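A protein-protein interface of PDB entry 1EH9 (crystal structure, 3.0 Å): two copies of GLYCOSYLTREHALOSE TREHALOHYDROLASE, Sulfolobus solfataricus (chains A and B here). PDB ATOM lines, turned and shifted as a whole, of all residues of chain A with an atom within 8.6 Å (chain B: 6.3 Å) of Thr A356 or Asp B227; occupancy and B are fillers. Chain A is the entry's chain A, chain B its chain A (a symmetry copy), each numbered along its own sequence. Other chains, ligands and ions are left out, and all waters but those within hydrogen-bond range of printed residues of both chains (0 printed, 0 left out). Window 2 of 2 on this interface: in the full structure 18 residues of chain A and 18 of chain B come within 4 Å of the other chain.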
ATOM      1  N   ASN A 287      19.887 -16.860  18.165  1.00  0.00           N
ATOM      2  CA  ASN A 287      19.662 -17.342  16.783  1.00  0.00           C
ATOM      3  C   ASN A 287      18.357 -18.022  16.621  1.00  0.00           C
ATOM      4  O   ASN A 287      18.268 -19.105  16.086  1.00  0.00           O
ATOM      5  CB  ASN A 287      20.776 -18.208  16.192  1.00  0.00           C
ATOM      6  CG  ASN A 287      22.007 -17.456  15.710  1.00  0.00           C
ATOM      7  OD1 ASN A 287      22.142 -16.201  15.832  1.00  0.00           O
ATOM      8  ND2 ASN A 287      22.835 -18.212  14.991  1.00  0.00           N
ATOM      9  N   TYR A 345      25.107 -20.121  13.132  1.00  0.00           N
ATOM     10  CA  TYR A 345      24.808 -20.923  14.321  1.00  0.00           C
ATOM     11  C   TYR A 345      23.343 -21.293  14.360  1.00  0.00           C
ATOM     12  O   TYR A 345      22.495 -20.572  14.890  1.00  0.00           O
ATOM     13  CB  TYR A 345      25.235 -20.270  15.618  1.00  0.00           C
ATOM     14  CG  TYR A 345      26.713 -20.314  15.634  1.00  0.00           C
ATOM     15  CD1 TYR A 345      27.434 -19.688  14.615  1.00  0.00           C
ATOM     16  CD2 TYR A 345      27.396 -21.037  16.605  1.00  0.00           C
ATOM     17  CE1 TYR A 345      28.820 -19.795  14.549  1.00  0.00           C
ATOM     18  CE2 TYR A 345      28.793 -21.113  16.588  1.00  0.00           C
ATOM     19  CZ  TYR A 345      29.493 -20.486  15.559  1.00  0.00           C
ATOM     20  OH  TYR A 345      30.843 -20.586  15.523  1.00  0.00           O
ATOM     21  N   ASP A 346      23.116 -22.417  13.708  1.00  0.00           N
ATOM     22  CA  ASP A 346      21.860 -23.039  13.498  1.00  0.00           C
ATOM     23  C   ASP A 346      21.684 -24.035  14.645  1.00  0.00           C
ATOM     24  O   ASP A 346      21.215 -25.159  14.510  1.00  0.00           O
ATOM     25  CB  ASP A 346      22.151 -23.824  12.197  1.00  0.00           C
ATOM     26  CG  ASP A 346      21.280 -23.371  11.085  1.00  0.00           C
ATOM     27  OD1 ASP A 346      20.734 -22.272  11.079  1.00  0.00           O
ATOM     28  OD2 ASP A 346      21.158 -24.288  10.145  1.00  0.00           O
ATOM     29  N   GLY A 347      22.199 -23.738  15.800  1.00  0.00           N
ATOM     30  CA  GLY A 347      22.084 -24.809  16.735  1.00  0.00           C
ATOM     31  C   GLY A 347      23.369 -25.582  16.780  1.00  0.00           C
ATOM     32  O   GLY A 347      23.428 -26.736  16.291  1.00  0.00           O
ATOM     33  N   LYS A 348      24.385 -24.920  17.370  1.00  0.00           N
ATOM     34  CA  LYS A 348      25.694 -25.550  17.437  1.00  0.00           C
ATOM     35  C   LYS A 348      26.605 -24.891  18.401  1.00  0.00           C
ATOM     36  O   LYS A 348      26.267 -23.848  18.951  1.00  0.00           O
ATOM     37  CB  LYS A 348      26.376 -25.748  16.108  1.00  0.00           C
ATOM     38  CG  LYS A 348      27.112 -24.512  15.591  1.00  0.00           C
ATOM     39  CD  LYS A 348      26.858 -24.263  14.109  1.00  0.00           C
ATOM     40  CE  LYS A 348      25.822 -25.227  13.534  1.00  0.00           C
ATOM     41  NZ  LYS A 348      24.780 -24.552  12.759  1.00  0.00           N
ATOM     42  N   TYR A 349      27.746 -25.524  18.629  1.00  0.00           N
ATOM     43  CA  TYR A 349      28.655 -25.006  19.631  1.00  0.00           C
ATOM     44  C   TYR A 349      29.448 -23.712  19.365  1.00  0.00           C
ATOM     45  O   TYR A 349      30.365 -23.643  18.562  1.00  0.00           O
ATOM     46  CB  TYR A 349      29.464 -26.099  20.395  1.00  0.00           C
ATOM     47  CG  TYR A 349      29.780 -25.732  21.836  1.00  0.00           C
ATOM     48  CD1 TYR A 349      30.102 -24.425  22.199  1.00  0.00           C
ATOM     49  CD2 TYR A 349      29.764 -26.698  22.838  1.00  0.00           C
ATOM     50  CE1 TYR A 349      30.371 -24.078  23.523  1.00  0.00           C
ATOM     51  CE2 TYR A 349      30.037 -26.374  24.166  1.00  0.00           C
ATOM     52  CZ  TYR A 349      30.336 -25.058  24.509  1.00  0.00           C
ATOM     53  OH  TYR A 349      30.620 -24.734  25.802  1.00  0.00           O
ATOM     54  N   SER A 350      29.142 -22.702  20.134  1.00  0.00           N
ATOM     55  CA  SER A 350      29.859 -21.492  20.087  1.00  0.00           C
ATOM     56  C   SER A 350      30.898 -21.496  21.181  1.00  0.00           C
ATOM     57  O   SER A 350      30.602 -21.251  22.332  1.00  0.00           O
ATOM     58  CB  SER A 350      28.968 -20.290  20.349  1.00  0.00           C
ATOM     59  OG  SER A 350      29.585 -19.462  21.348  1.00  0.00           O
ATOM     60  N   ASN A 351      32.159 -21.659  20.863  1.00  0.00           N
ATOM     61  CA  ASN A 351      33.112 -21.556  21.967  1.00  0.00           C
ATOM     62  C   ASN A 351      33.086 -20.143  22.466  1.00  0.00           C
ATOM     63  O   ASN A 351      33.564 -19.805  23.537  1.00  0.00           O
ATOM     64  CB  ASN A 351      34.550 -21.914  21.570  1.00  0.00           C
ATOM     65  CG  ASN A 351      34.592 -22.952  20.472  1.00  0.00           C
ATOM     66  OD1 ASN A 351      35.003 -24.103  20.709  1.00  0.00           O
ATOM     67  ND2 ASN A 351      34.085 -22.570  19.291  1.00  0.00           N
ATOM     68  N   ARG A 353      30.509 -18.402  23.233  1.00  0.00           N
ATOM     69  CA  ARG A 353      29.573 -18.337  24.322  1.00  0.00           C
ATOM     70  C   ARG A 353      29.605 -19.553  25.177  1.00  0.00           C
ATOM     71  O   ARG A 353      28.938 -19.601  26.189  1.00  0.00           O
ATOM     72  CB  ARG A 353      28.175 -18.201  23.787  1.00  0.00           C
ATOM     73  CG  ARG A 353      28.168 -17.381  22.527  1.00  0.00           C
ATOM     74  CD  ARG A 353      26.884 -17.521  21.741  1.00  0.00           C
ATOM     75  NE  ARG A 353      26.199 -16.240  21.651  1.00  0.00           N
ATOM     76  CZ  ARG A 353      26.114 -15.529  20.537  1.00  0.00           C
ATOM     77  NH1 ARG A 353      26.648 -15.926  19.368  1.00  0.00           N
ATOM     78  NH2 ARG A 353      25.474 -14.378  20.603  1.00  0.00           N
ATOM     79  N   ARG A 354      30.351 -20.537  24.750  1.00  0.00           N
ATOM     80  CA  ARG A 354      30.400 -21.779  25.493  1.00  0.00           C
ATOM     81  C   ARG A 354      28.974 -22.309  25.714  1.00  0.00           C
ATOM     82  O   ARG A 354      28.548 -22.800  26.780  1.00  0.00           O
ATOM     83  CB  ARG A 354      31.197 -21.681  26.775  1.00  0.00           C
ATOM     84  CG  ARG A 354      31.927 -20.362  26.980  1.00  0.00           C
ATOM     85  CD  ARG A 354      33.422 -20.630  27.127  1.00  0.00           C
ATOM     86  NE  ARG A 354      33.855 -21.777  26.307  1.00  0.00           N
ATOM     87  CZ  ARG A 354      33.853 -23.075  26.673  1.00  0.00           C
ATOM     88  NH1 ARG A 354      33.465 -23.496  27.877  1.00  0.00           N
ATOM     89  NH2 ARG A 354      34.272 -23.990  25.794  1.00  0.00           N
ATOM     90  N   LYS A 355      28.216 -22.192  24.666  1.00  0.00           N
ATOM     91  CA  LYS A 355      26.873 -22.606  24.763  1.00  0.00           C
ATOM     92  C   LYS A 355      26.491 -23.263  23.459  1.00  0.00           C
ATOM     93  O   LYS A 355      27.388 -23.562  22.708  1.00  0.00           O
ATOM     94  CB  LYS A 355      26.033 -21.427  25.276  1.00  0.00           C
ATOM     95  CG  LYS A 355      24.635 -21.337  24.738  1.00  0.00           C
ATOM     96  CD  LYS A 355      24.065 -19.966  24.937  1.00  0.00           C
ATOM     97  CE  LYS A 355      22.884 -19.726  24.014  1.00  0.00           C
ATOM     98  NZ  LYS A 355      22.536 -18.301  23.909  1.00  0.00           N
ATOM     99  N   THR A 356      25.231 -23.615  23.241  1.00  0.00           N
ATOM    100  CA  THR A 356      24.840 -24.296  22.014  1.00  0.00           C
ATOM    101  C   THR A 356      23.857 -23.404  21.374  1.00  0.00           C
ATOM    102  O   THR A 356      22.644 -23.490  21.616  1.00  0.00           O
ATOM    103  CB  THR A 356      24.280 -25.750  22.140  1.00  0.00           C
ATOM    104  OG1 THR A 356      25.294 -26.693  22.495  1.00  0.00           O
ATOM    105  CG2 THR A 356      23.621 -26.181  20.820  1.00  0.00           C
ATOM    106  N   HIS A 357      24.437 -22.514  20.597  1.00  0.00           N
ATOM    107  CA  HIS A 357      23.736 -21.431  19.984  1.00  0.00           C
ATOM    108  C   HIS A 357      22.876 -21.684  18.800  1.00  0.00           C
ATOM    109  O   HIS A 357      23.141 -22.558  17.962  1.00  0.00           O
ATOM    110  CB  HIS A 357      24.662 -20.267  19.805  1.00  0.00           C
ATOM    111  CG  HIS A 357      23.955 -19.009  19.724  1.00  0.00           C
ATOM    112  ND1 HIS A 357      22.930 -18.837  18.811  1.00  0.00           N
ATOM    113  CD2 HIS A 357      24.194 -17.847  20.349  1.00  0.00           C
ATOM    114  CE1 HIS A 357      22.506 -17.581  18.933  1.00  0.00           C
ATOM    115  NE2 HIS A 357      23.252 -16.968  19.854  1.00  0.00           N
ATOM    116  N   GLY A 358      21.825 -20.868  18.862  1.00  0.00           N
ATOM    117  CA  GLY A 358      20.727 -20.666  17.909  1.00  0.00           C
ATOM    118  C   GLY A 358      20.096 -21.902  17.337  1.00  0.00           C
ATOM    119  O   GLY A 358      20.294 -22.985  17.838  1.00  0.00           O
ATOM    120  N   GLU A 359      19.310 -21.706  16.290  1.00  0.00           N
ATOM    121  CA  GLU A 359      18.620 -22.790  15.650  1.00  0.00           C
ATOM    122  C   GLU A 359      18.057 -22.448  14.302  1.00  0.00           C
ATOM    123  O   GLU A 359      17.638 -21.335  14.050  1.00  0.00           O
ATOM    124  CB  GLU A 359      17.403 -23.167  16.494  1.00  0.00           C
ATOM    125  CG  GLU A 359      16.073 -23.065  15.698  1.00  0.00           C
ATOM    126  CD  GLU A 359      15.073 -24.184  15.959  1.00  0.00           C
ATOM    127  OE1 GLU A 359      15.390 -25.346  16.223  1.00  0.00           O
ATOM    128  OE2 GLU A 359      13.823 -23.781  15.810  1.00  0.00           O
ATOM    129  N   TYR B  42      35.170 -31.083  32.656  1.00  0.00           N
ATOM    130  CA  TYR B  42      34.936 -32.386  33.256  1.00  0.00           C
ATOM    131  C   TYR B  42      36.143 -33.161  33.724  1.00  0.00           C
ATOM    132  O   TYR B  42      36.693 -33.983  32.938  1.00  0.00           O
ATOM    133  CB  TYR B  42      34.245 -33.351  32.278  1.00  0.00           C
ATOM    134  CG  TYR B  42      32.833 -32.988  31.963  1.00  0.00           C
ATOM    135  CD1 TYR B  42      32.109 -32.163  32.821  1.00  0.00           C
ATOM    136  CD2 TYR B  42      32.235 -33.478  30.804  1.00  0.00           C
ATOM    137  CE1 TYR B  42      30.794 -31.821  32.521  1.00  0.00           C
ATOM    138  CE2 TYR B  42      30.925 -33.134  30.482  1.00  0.00           C
ATOM    139  CZ  TYR B  42      30.219 -32.295  31.342  1.00  0.00           C
ATOM    140  OH  TYR B  42      28.940 -31.950  31.034  1.00  0.00           O
ATOM    141  N   ASN B 220      21.113 -22.661  35.633  1.00  0.00           N
ATOM    142  CA  ASN B 220      21.532 -22.046  34.408  1.00  0.00           C
ATOM    143  C   ASN B 220      21.151 -22.813  33.185  1.00  0.00           C
ATOM    144  O   ASN B 220      21.924 -23.646  32.743  1.00  0.00           O
ATOM    145  CB  ASN B 220      23.044 -21.918  34.404  1.00  0.00           C
ATOM    146  CG  ASN B 220      23.430 -21.011  33.292  1.00  0.00           C
ATOM    147  OD1 ASN B 220      22.677 -20.063  32.982  1.00  0.00           O
ATOM    148  ND2 ASN B 220      24.474 -21.398  32.581  1.00  0.00           N
ATOM    149  N   PHE B 221      20.005 -22.497  32.606  1.00  0.00           N
ATOM    150  CA  PHE B 221      19.556 -23.227  31.411  1.00  0.00           C
ATOM    151  C   PHE B 221      19.815 -22.489  30.129  1.00  0.00           C
ATOM    152  O   PHE B 221      19.569 -23.030  29.050  1.00  0.00           O
ATOM    153  CB  PHE B 221      18.034 -23.418  31.502  1.00  0.00           C
ATOM    154  CG  PHE B 221      17.681 -23.961  32.859  1.00  0.00           C
ATOM    155  CD1 PHE B 221      17.629 -23.108  33.963  1.00  0.00           C
ATOM    156  CD2 PHE B 221      17.471 -25.331  33.035  1.00  0.00           C
ATOM    157  CE1 PHE B 221      17.337 -23.611  35.230  1.00  0.00           C
ATOM    158  CE2 PHE B 221      17.189 -25.855  34.290  1.00  0.00           C
ATOM    159  CZ  PHE B 221      17.140 -24.983  35.380  1.00  0.00           C
ATOM    160  N   ASP B 222      20.285 -21.240  30.324  1.00  0.00           N
ATOM    161  CA  ASP B 222      20.497 -20.176  29.353  1.00  0.00           C
ATOM    162  C   ASP B 222      21.926 -19.817  28.933  1.00  0.00           C
ATOM    163  O   ASP B 222      22.398 -20.239  27.885  1.00  0.00           O
ATOM    164  CB  ASP B 222      19.793 -18.937  29.936  1.00  0.00           C
ATOM    165  CG  ASP B 222      18.402 -18.933  29.439  1.00  0.00           C
ATOM    166  OD1 ASP B 222      17.934 -19.849  28.768  1.00  0.00           O
ATOM    167  OD2 ASP B 222      17.786 -17.819  29.688  1.00  0.00           O
ATOM    168  N   ASP B 223      22.570 -18.964  29.731  1.00  0.00           N
ATOM    169  CA  ASP B 223      23.912 -18.428  29.494  1.00  0.00           C
ATOM    170  C   ASP B 223      25.022 -19.471  29.463  1.00  0.00           C
ATOM    171  O   ASP B 223      24.835 -20.624  29.100  1.00  0.00           O
ATOM    172  CB  ASP B 223      24.267 -17.387  30.594  1.00  0.00           C
ATOM    173  CG  ASP B 223      24.375 -15.938  30.174  1.00  0.00           C
ATOM    174  OD1 ASP B 223      24.005 -15.494  29.083  1.00  0.00           O
ATOM    175  OD2 ASP B 223      24.877 -15.195  31.146  1.00  0.00           O
ATOM    176  N   ALA B 224      26.191 -18.987  29.864  1.00  0.00           N
ATOM    177  CA  ALA B 224      27.399 -19.740  30.018  1.00  0.00           C
ATOM    178  C   ALA B 224      27.322 -21.145  29.499  1.00  0.00           C
ATOM    179  O   ALA B 224      27.183 -21.375  28.302  1.00  0.00           O
ATOM    180  CB  ALA B 224      27.702 -19.819  31.492  1.00  0.00           C
ATOM    181  N   GLU B 225      27.455 -22.104  30.399  1.00  0.00           N
ATOM    182  CA  GLU B 225      27.450 -23.454  29.893  1.00  0.00           C
ATOM    183  C   GLU B 225      26.158 -24.254  30.053  1.00  0.00           C
ATOM    184  O   GLU B 225      26.168 -25.476  30.156  1.00  0.00           O
ATOM    185  CB  GLU B 225      28.720 -24.235  30.277  1.00  0.00           C
ATOM    186  CG  GLU B 225      30.032 -23.634  29.713  1.00  0.00           C
ATOM    187  CD  GLU B 225      31.010 -23.137  30.767  1.00  0.00           C
ATOM    188  OE1 GLU B 225      30.848 -22.113  31.420  1.00  0.00           O
ATOM    189  OE2 GLU B 225      32.101 -23.879  30.851  1.00  0.00           O
ATOM    190  N   SER B 226      25.031 -23.566  30.023  1.00  0.00           N
ATOM    191  CA  SER B 226      23.729 -24.203  30.151  1.00  0.00           C
ATOM    192  C   SER B 226      23.697 -25.667  29.689  1.00  0.00           C
ATOM    193  O   SER B 226      22.985 -26.511  30.241  1.00  0.00           O
ATOM    194  CB  SER B 226      22.698 -23.401  29.392  1.00  0.00           C
ATOM    195  OG  SER B 226      22.970 -23.549  28.010  1.00  0.00           O
ATOM    196  N   ASP B 227      24.441 -25.948  28.643  1.00  0.00           N
ATOM    197  CA  ASP B 227      24.508 -27.287  28.107  1.00  0.00           C
ATOM    198  C   ASP B 227      24.584 -28.350  29.212  1.00  0.00           C
ATOM    199  O   ASP B 227      23.761 -29.251  29.282  1.00  0.00           O
ATOM    200  CB  ASP B 227      25.739 -27.439  27.183  1.00  0.00           C
ATOM    201  CG  ASP B 227      25.907 -26.343  26.186  1.00  0.00           C
ATOM    202  OD1 ASP B 227      25.448 -26.429  25.058  1.00  0.00           O
ATOM    203  OD2 ASP B 227      26.671 -25.352  26.638  1.00  0.00           O
ATOM    204  N   GLU B 228      25.649 -28.244  30.010  1.00  0.00           N
ATOM    205  CA  GLU B 228      25.974 -29.108  31.120  1.00  0.00           C
ATOM    206  C   GLU B 228      24.867 -29.100  32.188  1.00  0.00           C
ATOM    207  O   GLU B 228      24.288 -30.153  32.468  1.00  0.00           O
ATOM    208  CB  GLU B 228      27.368 -28.736  31.698  1.00  0.00           C
ATOM    209  CG  GLU B 228      28.538 -29.191  30.796  1.00  0.00           C
ATOM    210  CD  GLU B 228      28.303 -29.028  29.295  1.00  0.00           C
ATOM    211  OE1 GLU B 228      28.544 -27.991  28.675  1.00  0.00           O
ATOM    212  OE2 GLU B 228      27.922 -30.143  28.697  1.00  0.00           O
ATOM    213  N   VAL B 229      24.557 -27.919  32.772  1.00  0.00           N
ATOM    214  CA  VAL B 229      23.496 -27.866  33.744  1.00  0.00           C
ATOM    215  C   VAL B 229      22.205 -28.378  33.162  1.00  0.00           C
ATOM    216  O   VAL B 229      21.495 -29.170  33.727  1.00  0.00           O
ATOM    217  CB  VAL B 229      23.289 -26.562  34.514  1.00  0.00           C
ATOM    218  CG1 VAL B 229      24.348 -25.545  34.217  1.00  0.00           C
ATOM    219  CG2 VAL B 229      21.916 -25.991  34.265  1.00  0.00           C
ATOM    220  N   ARG B 230      21.880 -27.976  31.997  1.00  0.00           N
ATOM    221  CA  ARG B 230      20.656 -28.504  31.510  1.00  0.00           C
ATOM    222  C   ARG B 230      20.745 -29.995  31.167  1.00  0.00           C
ATOM    223  O   ARG B 230      19.766 -30.635  30.811  1.00  0.00           O
ATOM    224  CB  ARG B 230      20.082 -27.623  30.422  1.00  0.00           C
ATOM    225  CG  ARG B 230      20.758 -27.787  29.084  1.00  0.00           C
ATOM    226  CD  ARG B 230      19.784 -27.466  27.967  1.00  0.00           C
ATOM    227  NE  ARG B 230      19.098 -26.223  28.278  1.00  0.00           N
ATOM    228  CZ  ARG B 230      17.924 -25.920  27.726  1.00  0.00           C
ATOM    229  NH1 ARG B 230      17.314 -26.729  26.848  1.00  0.00           N
ATOM    230  NH2 ARG B 230      17.339 -24.775  28.070  1.00  0.00           N
ATOM    231  N   LYS B 231      21.924 -30.584  31.274  1.00  0.00           N
ATOM    232  CA  LYS B 231      22.018 -32.010  30.969  1.00  0.00           C
ATOM    233  C   LYS B 231      21.849 -32.738  32.268  1.00  0.00           C
ATOM    234  O   LYS B 231      21.137 -33.726  32.371  1.00  0.00           O
ATOM    235  CB  LYS B 231      23.288 -32.448  30.243  1.00  0.00           C
ATOM    236  N   PHE B 232      22.484 -32.181  33.287  1.00  0.00           N
ATOM    237  CA  PHE B 232      22.344 -32.701  34.623  1.00  0.00           C
ATOM    238  C   PHE B 232      20.953 -33.236  34.767  1.00  0.00           C
ATOM    239  O   PHE B 232      20.656 -34.431  34.914  1.00  0.00           O
ATOM    240  CB  PHE B 232      22.292 -31.514  35.581  1.00  0.00           C
ATOM    241  CG  PHE B 232      22.928 -31.864  36.858  1.00  0.00           C
ATOM    242  CD1 PHE B 232      23.442 -33.145  37.045  1.00  0.00           C
ATOM    243  CD2 PHE B 232      23.082 -30.917  37.869  1.00  0.00           C
ATOM    244  CE1 PHE B 232      24.100 -33.472  38.231  1.00  0.00           C
ATOM    245  CE2 PHE B 232      23.727 -31.230  39.068  1.00  0.00           C
ATOM    246  CZ  PHE B 232      24.240 -32.515  39.241  1.00  0.00           C
ATOM    247  N   PRO B 262      15.689 -21.743  22.443  1.00  0.00           N
ATOM    248  CA  PRO B 262      14.595 -21.939  21.500  1.00  0.00           C
ATOM    249  C   PRO B 262      13.683 -23.071  21.900  1.00  0.00           C
ATOM    250  O   PRO B 262      12.533 -23.145  21.463  1.00  0.00           O
ATOM    251  CB  PRO B 262      15.188 -22.089  20.106  1.00  0.00           C
ATOM    252  CG  PRO B 262      16.665 -21.738  20.250  1.00  0.00           C
ATOM    253  CD  PRO B 262      16.914 -21.358  21.707  1.00  0.00           C
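O of Arg A353 sits close to O of Ala B224 (3.3 Å). OD1 of Asp B227 is in hydrogen-bond range of OG1 of Thr A356 (2.6 Å). The side-chain carboxylate of Asp B227 lies close to the backbone carbonyl oxygen of Arg A354, at 3.2 Å. NH1 of Arg A354 lies within salt-bridge range of OE2 of Glu B225, at 3.3 Å. O of Arg A354 lies close to O of Ala B224 (2.5 Å).
O of Asp B222 sits at hydrogen-bond distance from OG of Ser B226, 3.4 Å away. The guanidinium group (NE) of Arg A354 lies within hydrogen-bond range of the backbone carbonyl oxygen (O) of Asn A351 (3.4 Å). OH of Tyr A349 sits close to O of Arg A354, at 3.0 Å. The backbone NH (N) of Ser A350 lies within hydrogen-bond range of the backbone carbonyl oxygen (O) of Lys A355. A ring nitrogen (NE2) of His A357 sits close to the guanidinium group of Arg A353 (3.5 Å).
Asp B222 touches Lys A355 (O to CD, 3.4 Å). Lys A355 touches Ala B224. CA of Lys A355 touches OD2 of Asp B227, 3.3 Å away.
Ser A350 touches none of the printed residues of chain B. Of the printed residues of chain B, Arg A353 touches Ala B224. Of the printed residues of chain B, Arg A354 touches Ala B224 (2.5 Å), Glu B225 (3.3 Å) and Asp B227 (3.2 Å). Printed residues of chain B within 4 Å of Lys A355: Asp B222, Ala B224 and Asp B227. Printed residues of chain A within 4 Å of Asp B222: Lys A355 (3.4 Å). Of the printed residues of chain A, Ala B224 touches Arg A353 (3.3 Å), Arg A354 (2.5 Å) and Lys A355 (3.2 Å). No residue of chain A comes within 4 Å of Ser B226. Of chain A, only Arg A354 (3.2 Å), Lys A355 (3.3 Å) and Thr A356 (2.6 Å) come within 4 Å of Asp B227. No residue of chain A comes within 4 Å of Glu B228. The nearest printed residue of chain A that does not touch Asp B222 is Thr A356 (6.4 Å).
Of the 15 printed residues of chain A, 4 touch a printed residue of chain B. Among the printed residues, Asp or Glu carboxylates within 4 Å of a Lys or Arg side-chain nitrogen of the other chain: Arg A354 with Glu B225.
No position is printed for both chains.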
